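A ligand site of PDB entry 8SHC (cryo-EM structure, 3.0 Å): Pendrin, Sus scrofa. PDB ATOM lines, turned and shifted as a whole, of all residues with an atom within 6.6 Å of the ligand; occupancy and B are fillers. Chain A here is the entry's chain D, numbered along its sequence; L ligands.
The side-chain hydroxyl (OH) of Tyr 105 is in hydrogen-bond range of an oxygen (O1) of the ligand, 2.9 Å away. The side-chain amide nitrogen of Asn 457 lies close to an oxygen (O2) of the ligand (3.4 Å).
A fluorine (F1) of the ligand sits close to the side-chain carboxylate of Glu 303 (2.8 Å). Val 97 touches the ligand (CG2 to F3, 3.3 Å). Gln 101 touches the ligand (CG to C8, 3.8 Å). Ala 104 touches the ligand (CB to C12, 3.8 Å). CA of Pro 301 touches F1 of the ligand, at 3.3 Å. Val 304 touches the ligand (CG2 to F2, 3.6 Å). Ser 408 touches the ligand. Val 453 touches the ligand. Hydrophobic or aromatic side chains that line the ligand: Val 97, Ala 104, Tyr 105, Pro 301, Val 304 and Val 453. Ten residues have an atom within 4 Å of the ligand: Val 97, Gln 101, Ala 104, Tyr 105, Pro 301, Glu 303, Val 304, Ser 408, Val 453 and Asn 457.
The side-chain amino group (NZ) of Lys 286 is in salt-bridge range of the side-chain carboxylate (OE2) of Glu 303 (2.5 Å). The backbone carbonyl oxygen (O) of Glu 303 lies within hydrogen-bond range of the side-chain hydroxyl (OG1) of Thr 307 (3.2 Å). OH of Tyr 105 is in hydrogen-bond range of NE2 of Gln 101, 2.8 Å away. O of Val 453 lies within hydrogen-bond range of ND2 of Asn 457, at 3.0 Å. NH1 of Arg 409 lies close to OE1 of Gln 101, 3.4 Å away.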
ATOM      1  N   SER A  93      -8.284  17.304 -35.186  1.00  0.00           N
ATOM      2  CA  SER A  93      -8.578  18.113 -34.010  1.00  0.00           C
ATOM      3  C   SER A  93      -9.322  17.306 -32.953  1.00  0.00           C
ATOM      4  O   SER A  93      -8.962  17.307 -31.763  1.00  0.00           O
ATOM      5  CB  SER A  93      -9.365  19.364 -34.405  1.00  0.00           C
ATOM      6  OG  SER A  93      -8.765  20.021 -35.503  1.00  0.00           O
ATOM      7  N   LEU A  96      -7.077  14.731 -31.266  1.00  0.00           N
ATOM      8  CA  LEU A  96      -6.212  15.359 -30.279  1.00  0.00           C
ATOM      9  C   LEU A  96      -6.969  15.648 -28.987  1.00  0.00           C
ATOM     10  O   LEU A  96      -6.442  15.463 -27.897  1.00  0.00           O
ATOM     11  CB  LEU A  96      -5.596  16.632 -30.843  1.00  0.00           C
ATOM     12  CG  LEU A  96      -4.614  16.469 -32.005  1.00  0.00           C
ATOM     13  CD1 LEU A  96      -4.202  17.836 -32.539  1.00  0.00           C
ATOM     14  CD2 LEU A  96      -3.399  15.666 -31.584  1.00  0.00           C
ATOM     15  N   VAL A  97      -8.212  16.116 -29.112  1.00  0.00           N
ATOM     16  CA  VAL A  97      -9.011  16.352 -27.905  1.00  0.00           C
ATOM     17  C   VAL A  97      -9.411  15.029 -27.231  1.00  0.00           C
ATOM     18  O   VAL A  97      -9.344  14.914 -25.992  1.00  0.00           O
ATOM     19  CB  VAL A  97     -10.242  17.209 -28.240  1.00  0.00           C
ATOM     20  CG1 VAL A  97     -11.174  17.297 -27.047  1.00  0.00           C
ATOM     21  CG2 VAL A  97      -9.816  18.597 -28.688  1.00  0.00           C
ATOM     22  N   LEU A 100      -6.759  13.087 -24.912  1.00  0.00           N
ATOM     23  CA  LEU A 100      -6.664  13.646 -23.558  1.00  0.00           C
ATOM     24  C   LEU A 100      -7.926  13.389 -22.759  1.00  0.00           C
ATOM     25  O   LEU A 100      -7.851  13.084 -21.560  1.00  0.00           O
ATOM     26  CB  LEU A 100      -6.350  15.145 -23.625  1.00  0.00           C
ATOM     27  CG  LEU A 100      -4.895  15.581 -23.781  1.00  0.00           C
ATOM     28  CD1 LEU A 100      -4.079  15.152 -22.570  1.00  0.00           C
ATOM     29  CD2 LEU A 100      -4.266  15.068 -25.072  1.00  0.00           C
ATOM     30  N   GLN A 101      -9.093  13.524 -23.381  1.00  0.00           N
ATOM     31  CA  GLN A 101     -10.329  13.260 -22.651  1.00  0.00           C
ATOM     32  C   GLN A 101     -10.434  11.796 -22.195  1.00  0.00           C
ATOM     33  O   GLN A 101     -10.858  11.543 -21.064  1.00  0.00           O
ATOM     34  CB  GLN A 101     -11.553  13.629 -23.493  1.00  0.00           C
ATOM     35  CG  GLN A 101     -11.944  15.087 -23.386  1.00  0.00           C
ATOM     36  CD  GLN A 101     -13.209  15.411 -24.156  1.00  0.00           C
ATOM     37  OE1 GLN A 101     -13.242  15.309 -25.374  1.00  0.00           O
ATOM     38  NE2 GLN A 101     -14.250  15.799 -23.436  1.00  0.00           N
ATOM     39  N   GLY A 102     -10.054  10.844 -23.045  1.00  0.00           N
ATOM     40  CA  GLY A 102     -10.082   9.452 -22.642  1.00  0.00           C
ATOM     41  C   GLY A 102      -9.074   9.152 -21.547  1.00  0.00           C
ATOM     42  O   GLY A 102      -9.362   8.378 -20.622  1.00  0.00           O
ATOM     43  N   ALA A 104      -8.106  11.283 -19.284  1.00  0.00           N
ATOM     44  CA  ALA A 104      -8.597  11.899 -18.057  1.00  0.00           C
ATOM     45  C   ALA A 104      -9.767  11.120 -17.464  1.00  0.00           C
ATOM     46  O   ALA A 104      -9.819  10.909 -16.244  1.00  0.00           O
ATOM     47  CB  ALA A 104      -9.012  13.347 -18.332  1.00  0.00           C
ATOM     48  N   TYR A 105     -10.706  10.678 -18.299  1.00  0.00           N
ATOM     49  CA  TYR A 105     -11.896   9.991 -17.804  1.00  0.00           C
ATOM     50  C   TYR A 105     -11.610   8.587 -17.307  1.00  0.00           C
ATOM     51  O   TYR A 105     -12.485   7.991 -16.666  1.00  0.00           O
ATOM     52  CB  TYR A 105     -12.967   9.933 -18.896  1.00  0.00           C
ATOM     53  CG  TYR A 105     -13.405  11.296 -19.405  1.00  0.00           C
ATOM     54  CD1 TYR A 105     -13.367  12.409 -18.588  1.00  0.00           C
ATOM     55  CD2 TYR A 105     -13.872  11.448 -20.708  1.00  0.00           C
ATOM     56  CE1 TYR A 105     -13.767  13.644 -19.044  1.00  0.00           C
ATOM     57  CE2 TYR A 105     -14.275  12.684 -21.181  1.00  0.00           C
ATOM     58  CZ  TYR A 105     -14.222  13.778 -20.343  1.00  0.00           C
ATOM     59  OH  TYR A 105     -14.625  15.005 -20.805  1.00  0.00           O
ATOM     60  N   PRO A 142     -17.578  11.602 -18.628  1.00  0.00           N
ATOM     61  CA  PRO A 142     -17.223  11.116 -17.286  1.00  0.00           C
ATOM     62  C   PRO A 142     -18.346  10.736 -16.324  1.00  0.00           C
ATOM     63  O   PRO A 142     -18.062  10.088 -15.319  1.00  0.00           O
ATOM     64  CB  PRO A 142     -16.408  12.280 -16.715  1.00  0.00           C
ATOM     65  CG  PRO A 142     -16.955  13.483 -17.417  1.00  0.00           C
ATOM     66  CD  PRO A 142     -17.194  13.010 -18.819  1.00  0.00           C
ATOM     67  N   LYS A 286     -11.029  30.288 -19.986  1.00  0.00           N
ATOM     68  CA  LYS A 286     -12.395  30.048 -20.420  1.00  0.00           C
ATOM     69  C   LYS A 286     -13.268  31.289 -20.252  1.00  0.00           C
ATOM     70  O   LYS A 286     -14.122  31.578 -21.098  1.00  0.00           O
ATOM     71  CB  LYS A 286     -12.995  28.854 -19.662  1.00  0.00           C
ATOM     72  CG  LYS A 286     -12.698  27.517 -20.299  1.00  0.00           C
ATOM     73  CD  LYS A 286     -13.037  26.367 -19.368  1.00  0.00           C
ATOM     74  CE  LYS A 286     -13.374  25.106 -20.143  1.00  0.00           C
ATOM     75  NZ  LYS A 286     -12.411  24.870 -21.254  1.00  0.00           N
ATOM     76  N   PRO A 299     -12.740  26.970 -30.287  1.00  0.00           N
ATOM     77  CA  PRO A 299     -12.321  27.171 -28.891  1.00  0.00           C
ATOM     78  C   PRO A 299     -10.808  27.122 -28.751  1.00  0.00           C
ATOM     79  O   PRO A 299     -10.123  26.378 -29.455  1.00  0.00           O
ATOM     80  CB  PRO A 299     -12.999  26.002 -28.157  1.00  0.00           C
ATOM     81  CG  PRO A 299     -13.339  25.011 -29.216  1.00  0.00           C
ATOM     82  CD  PRO A 299     -13.630  25.807 -30.446  1.00  0.00           C
ATOM     83  N   ILE A 300     -10.300  27.917 -27.827  1.00  0.00           N
ATOM     84  CA  ILE A 300      -8.851  27.962 -27.570  1.00  0.00           C
ATOM     85  C   ILE A 300      -8.464  26.700 -26.805  1.00  0.00           C
ATOM     86  O   ILE A 300      -9.027  26.438 -25.733  1.00  0.00           O
ATOM     87  CB  ILE A 300      -8.479  29.221 -26.805  1.00  0.00           C
ATOM     88  CG1 ILE A 300      -8.526  30.437 -27.726  1.00  0.00           C
ATOM     89  CG2 ILE A 300      -7.092  29.072 -26.188  1.00  0.00           C
ATOM     90  CD1 ILE A 300      -7.524  30.377 -28.862  1.00  0.00           C
ATOM     91  N   PRO A 301      -7.507  25.910 -27.306  1.00  0.00           N
ATOM     92  CA  PRO A 301      -7.113  24.665 -26.617  1.00  0.00           C
ATOM     93  C   PRO A 301      -6.175  24.916 -25.447  1.00  0.00           C
ATOM     94  O   PRO A 301      -4.993  24.527 -25.439  1.00  0.00           O
ATOM     95  CB  PRO A 301      -6.451  23.870 -27.752  1.00  0.00           C
ATOM     96  CG  PRO A 301      -5.844  24.925 -28.616  1.00  0.00           C
ATOM     97  CD  PRO A 301      -6.778  26.109 -28.571  1.00  0.00           C
ATOM     98  N   ILE A 302      -6.697  25.593 -24.423  1.00  0.00           N
ATOM     99  CA  ILE A 302      -5.887  25.893 -23.241  1.00  0.00           C
ATOM    100  C   ILE A 302      -5.527  24.615 -22.496  1.00  0.00           C
ATOM    101  O   ILE A 302      -4.438  24.495 -21.934  1.00  0.00           O
ATOM    102  CB  ILE A 302      -6.619  26.896 -22.338  1.00  0.00           C
ATOM    103  CG1 ILE A 302      -5.793  27.188 -21.082  1.00  0.00           C
ATOM    104  CG2 ILE A 302      -8.006  26.389 -21.961  1.00  0.00           C
ATOM    105  CD1 ILE A 302      -4.469  27.868 -21.379  1.00  0.00           C
ATOM    106  N   GLU A 303      -6.430  23.635 -22.488  1.00  0.00           N
ATOM    107  CA  GLU A 303      -6.200  22.399 -21.737  1.00  0.00           C
ATOM    108  C   GLU A 303      -5.007  21.634 -22.284  1.00  0.00           C
ATOM    109  O   GLU A 303      -4.180  21.108 -21.522  1.00  0.00           O
ATOM    110  CB  GLU A 303      -7.451  21.534 -21.761  1.00  0.00           C
ATOM    111  CG  GLU A 303      -8.551  22.016 -20.825  1.00  0.00           C
ATOM    112  CD  GLU A 303      -9.477  23.019 -21.488  1.00  0.00           C
ATOM    113  OE1 GLU A 303      -9.257  23.351 -22.671  1.00  0.00           O
ATOM    114  OE2 GLU A 303     -10.429  23.476 -20.823  1.00  0.00           O
ATOM    115  N   VAL A 304      -4.888  21.540 -23.614  1.00  0.00           N
ATOM    116  CA  VAL A 304      -3.785  20.808 -24.224  1.00  0.00           C
ATOM    117  C   VAL A 304      -2.458  21.492 -23.904  1.00  0.00           C
ATOM    118  O   VAL A 304      -1.464  20.827 -23.571  1.00  0.00           O
ATOM    119  CB  VAL A 304      -4.007  20.679 -25.746  1.00  0.00           C
ATOM    120  CG1 VAL A 304      -2.745  20.197 -26.434  1.00  0.00           C
ATOM    121  CG2 VAL A 304      -5.167  19.744 -26.030  1.00  0.00           C
ATOM    122  N   ILE A 305      -2.421  22.812 -23.997  1.00  0.00           N
ATOM    123  CA  ILE A 305      -1.209  23.560 -23.688  1.00  0.00           C
ATOM    124  C   ILE A 305      -0.820  23.371 -22.225  1.00  0.00           C
ATOM    125  O   ILE A 305       0.359  23.192 -21.887  1.00  0.00           O
ATOM    126  CB  ILE A 305      -1.397  25.048 -24.042  1.00  0.00           C
ATOM    127  CG1 ILE A 305      -1.512  25.232 -25.557  1.00  0.00           C
ATOM    128  CG2 ILE A 305      -0.254  25.891 -23.499  1.00  0.00           C
ATOM    129  CD1 ILE A 305      -2.404  26.375 -25.961  1.00  0.00           C
ATOM    130  N   THR A 307      -1.551  20.817 -20.298  1.00  0.00           N
ATOM    131  CA  THR A 307      -1.057  19.454 -20.128  1.00  0.00           C
ATOM    132  C   THR A 307       0.376  19.308 -20.641  1.00  0.00           C
ATOM    133  O   THR A 307       1.211  18.688 -19.977  1.00  0.00           O
ATOM    134  CB  THR A 307      -1.978  18.468 -20.846  1.00  0.00           C
ATOM    135  OG1 THR A 307      -3.246  18.418 -20.165  1.00  0.00           O
ATOM    136  CG2 THR A 307      -1.371  17.077 -20.878  1.00  0.00           C
ATOM    137  N   SER A 408     -19.267  18.167 -25.577  1.00  0.00           N
ATOM    138  CA  SER A 408     -18.128  19.087 -25.705  1.00  0.00           C
ATOM    139  C   SER A 408     -17.227  18.689 -26.868  1.00  0.00           C
ATOM    140  O   SER A 408     -16.895  19.511 -27.739  1.00  0.00           O
ATOM    141  CB  SER A 408     -17.341  19.131 -24.398  1.00  0.00           C
ATOM    142  OG  SER A 408     -16.185  19.938 -24.534  1.00  0.00           O
ATOM    143  N   ARG A 409     -16.811  17.415 -26.906  1.00  0.00           N
ATOM    144  CA  ARG A 409     -15.968  16.958 -28.006  1.00  0.00           C
ATOM    145  C   ARG A 409     -16.731  16.976 -29.319  1.00  0.00           C
ATOM    146  O   ARG A 409     -16.140  17.187 -30.385  1.00  0.00           O
ATOM    147  CB  ARG A 409     -15.448  15.555 -27.707  1.00  0.00           C
ATOM    148  CG  ARG A 409     -14.437  15.039 -28.720  1.00  0.00           C
ATOM    149  CD  ARG A 409     -13.933  13.673 -28.313  1.00  0.00           C
ATOM    150  NE  ARG A 409     -15.058  12.750 -28.187  1.00  0.00           N
ATOM    151  CZ  ARG A 409     -15.396  12.137 -27.067  1.00  0.00           C
ATOM    152  NH1 ARG A 409     -14.697  12.287 -25.953  1.00  0.00           N
ATOM    153  NH2 ARG A 409     -16.482  11.368 -27.054  1.00  0.00           N
ATOM    154  N   VAL A 412     -16.413  20.428 -30.517  1.00  0.00           N
ATOM    155  CA  VAL A 412     -15.053  20.632 -31.010  1.00  0.00           C
ATOM    156  C   VAL A 412     -14.905  20.047 -32.413  1.00  0.00           C
ATOM    157  O   VAL A 412     -14.304  20.670 -33.298  1.00  0.00           O
ATOM    158  CB  VAL A 412     -14.030  20.023 -30.037  1.00  0.00           C
ATOM    159  CG1 VAL A 412     -12.630  20.063 -30.630  1.00  0.00           C
ATOM    160  CG2 VAL A 412     -14.069  20.762 -28.704  1.00  0.00           C
ATOM    161  N   LEU A 450      -5.059  16.158 -14.622  1.00  0.00           N
ATOM    162  CA  LEU A 450      -6.271  15.655 -15.269  1.00  0.00           C
ATOM    163  C   LEU A 450      -7.491  15.869 -14.377  1.00  0.00           C
ATOM    164  O   LEU A 450      -8.563  16.290 -14.852  1.00  0.00           O
ATOM    165  CB  LEU A 450      -6.108  14.178 -15.610  1.00  0.00           C
ATOM    166  CG  LEU A 450      -4.859  13.792 -16.402  1.00  0.00           C
ATOM    167  CD1 LEU A 450      -4.568  12.310 -16.259  1.00  0.00           C
ATOM    168  CD2 LEU A 450      -5.008  14.171 -17.857  1.00  0.00           C
ATOM    169  N   VAL A 453      -8.486  19.517 -14.562  1.00  0.00           N
ATOM    170  CA  VAL A 453      -9.248  19.830 -15.774  1.00  0.00           C
ATOM    171  C   VAL A 453     -10.691  19.355 -15.639  1.00  0.00           C
ATOM    172  O   VAL A 453     -11.640  20.076 -15.975  1.00  0.00           O
ATOM    173  CB  VAL A 453      -8.567  19.233 -17.006  1.00  0.00           C
ATOM    174  CG1 VAL A 453      -9.247  19.741 -18.266  1.00  0.00           C
ATOM    175  CG2 VAL A 453      -7.097  19.618 -17.050  1.00  0.00           C
ATOM    176  N   VAL A 454     -10.876  18.131 -15.150  1.00  0.00           N
ATOM    177  CA  VAL A 454     -12.230  17.595 -14.982  1.00  0.00           C
ATOM    178  C   VAL A 454     -13.043  18.482 -14.052  1.00  0.00           C
ATOM    179  O   VAL A 454     -14.217  18.769 -14.316  1.00  0.00           O
ATOM    180  CB  VAL A 454     -12.182  16.138 -14.469  1.00  0.00           C
ATOM    181  CG1 VAL A 454     -13.586  15.620 -14.207  1.00  0.00           C
ATOM    182  CG2 VAL A 454     -11.483  15.247 -15.491  1.00  0.00           C
ATOM    183  N   ILE A 455     -12.435  18.942 -12.958  1.00  0.00           N
ATOM    184  CA  ILE A 455     -13.124  19.847 -12.042  1.00  0.00           C
ATOM    185  C   ILE A 455     -13.431  21.176 -12.721  1.00  0.00           C
ATOM    186  O   ILE A 455     -14.519  21.744 -12.558  1.00  0.00           O
ATOM    187  CB  ILE A 455     -12.309  20.040 -10.755  1.00  0.00           C
ATOM    188  CG1 ILE A 455     -12.280  18.751  -9.934  1.00  0.00           C
ATOM    189  CG2 ILE A 455     -12.864  21.178  -9.920  1.00  0.00           C
ATOM    190  CD1 ILE A 455     -11.406  18.821  -8.707  1.00  0.00           C
ATOM    191  N   ASN A 457     -14.077  21.818 -15.732  1.00  0.00           N
ATOM    192  CA  ASN A 457     -15.158  21.737 -16.707  1.00  0.00           C
ATOM    193  C   ASN A 457     -16.523  21.435 -16.084  1.00  0.00           C
ATOM    194  O   ASN A 457     -17.399  20.913 -16.785  1.00  0.00           O
ATOM    195  CB  ASN A 457     -14.837  20.677 -17.765  1.00  0.00           C
ATOM    196  CG  ASN A 457     -13.875  21.171 -18.823  1.00  0.00           C
ATOM    197  OD1 ASN A 457     -14.272  21.869 -19.753  1.00  0.00           O
ATOM    198  ND2 ASN A 457     -12.602  20.826 -18.667  1.00  0.00           N
HETATM  199  F1  LIG L   1      -8.781  22.248 -25.224  1.00  0.00           F
HETATM  200  C1  LIG L   1      -9.507  21.210 -25.654  1.00  0.00           C
HETATM  201  F2  LIG L   1      -8.736  20.131 -25.529  1.00  0.00           F
HETATM  202  F3  LIG L   1      -9.672  21.401 -26.959  1.00  0.00           F
HETATM  203  C2  LIG L   1     -10.802  21.076 -24.922  1.00  0.00           C
HETATM  204  C3  LIG L   1     -10.911  20.175 -23.856  1.00  0.00           C
HETATM  205  C4  LIG L   1     -12.107  20.059 -23.164  1.00  0.00           C
HETATM  206  C5  LIG L   1     -13.203  20.841 -23.531  1.00  0.00           C
HETATM  207  C6  LIG L   1     -13.094  21.733 -24.585  1.00  0.00           C
HETATM  208  C7  LIG L   1     -11.897  21.849 -25.277  1.00  0.00           C
HETATM  209  N1  LIG L   1     -12.278  19.163 -22.084  1.00  0.00           N
HETATM  210  C8  LIG L   1     -11.439  18.323 -21.402  1.00  0.00           C
HETATM  211  N2  LIG L   1     -10.154  18.247 -21.806  1.00  0.00           N
HETATM  212  C9  LIG L   1     -11.942  17.559 -20.315  1.00  0.00           C
HETATM  213  C10 LIG L   1     -13.364  17.622 -19.848  1.00  0.00           C
HETATM  214  O1  LIG L   1     -13.691  16.911 -18.857  1.00  0.00           O
HETATM  215  O2  LIG L   1     -14.160  18.367 -20.470  1.00  0.00           O
HETATM  216  C11 LIG L   1     -11.049  16.710 -19.658  1.00  0.00           C
HETATM  217  C12 LIG L   1      -9.730  16.642 -20.083  1.00  0.00           C
HETATM  218  C13 LIG L   1      -9.338  17.415 -21.144  1.00  0.00           C
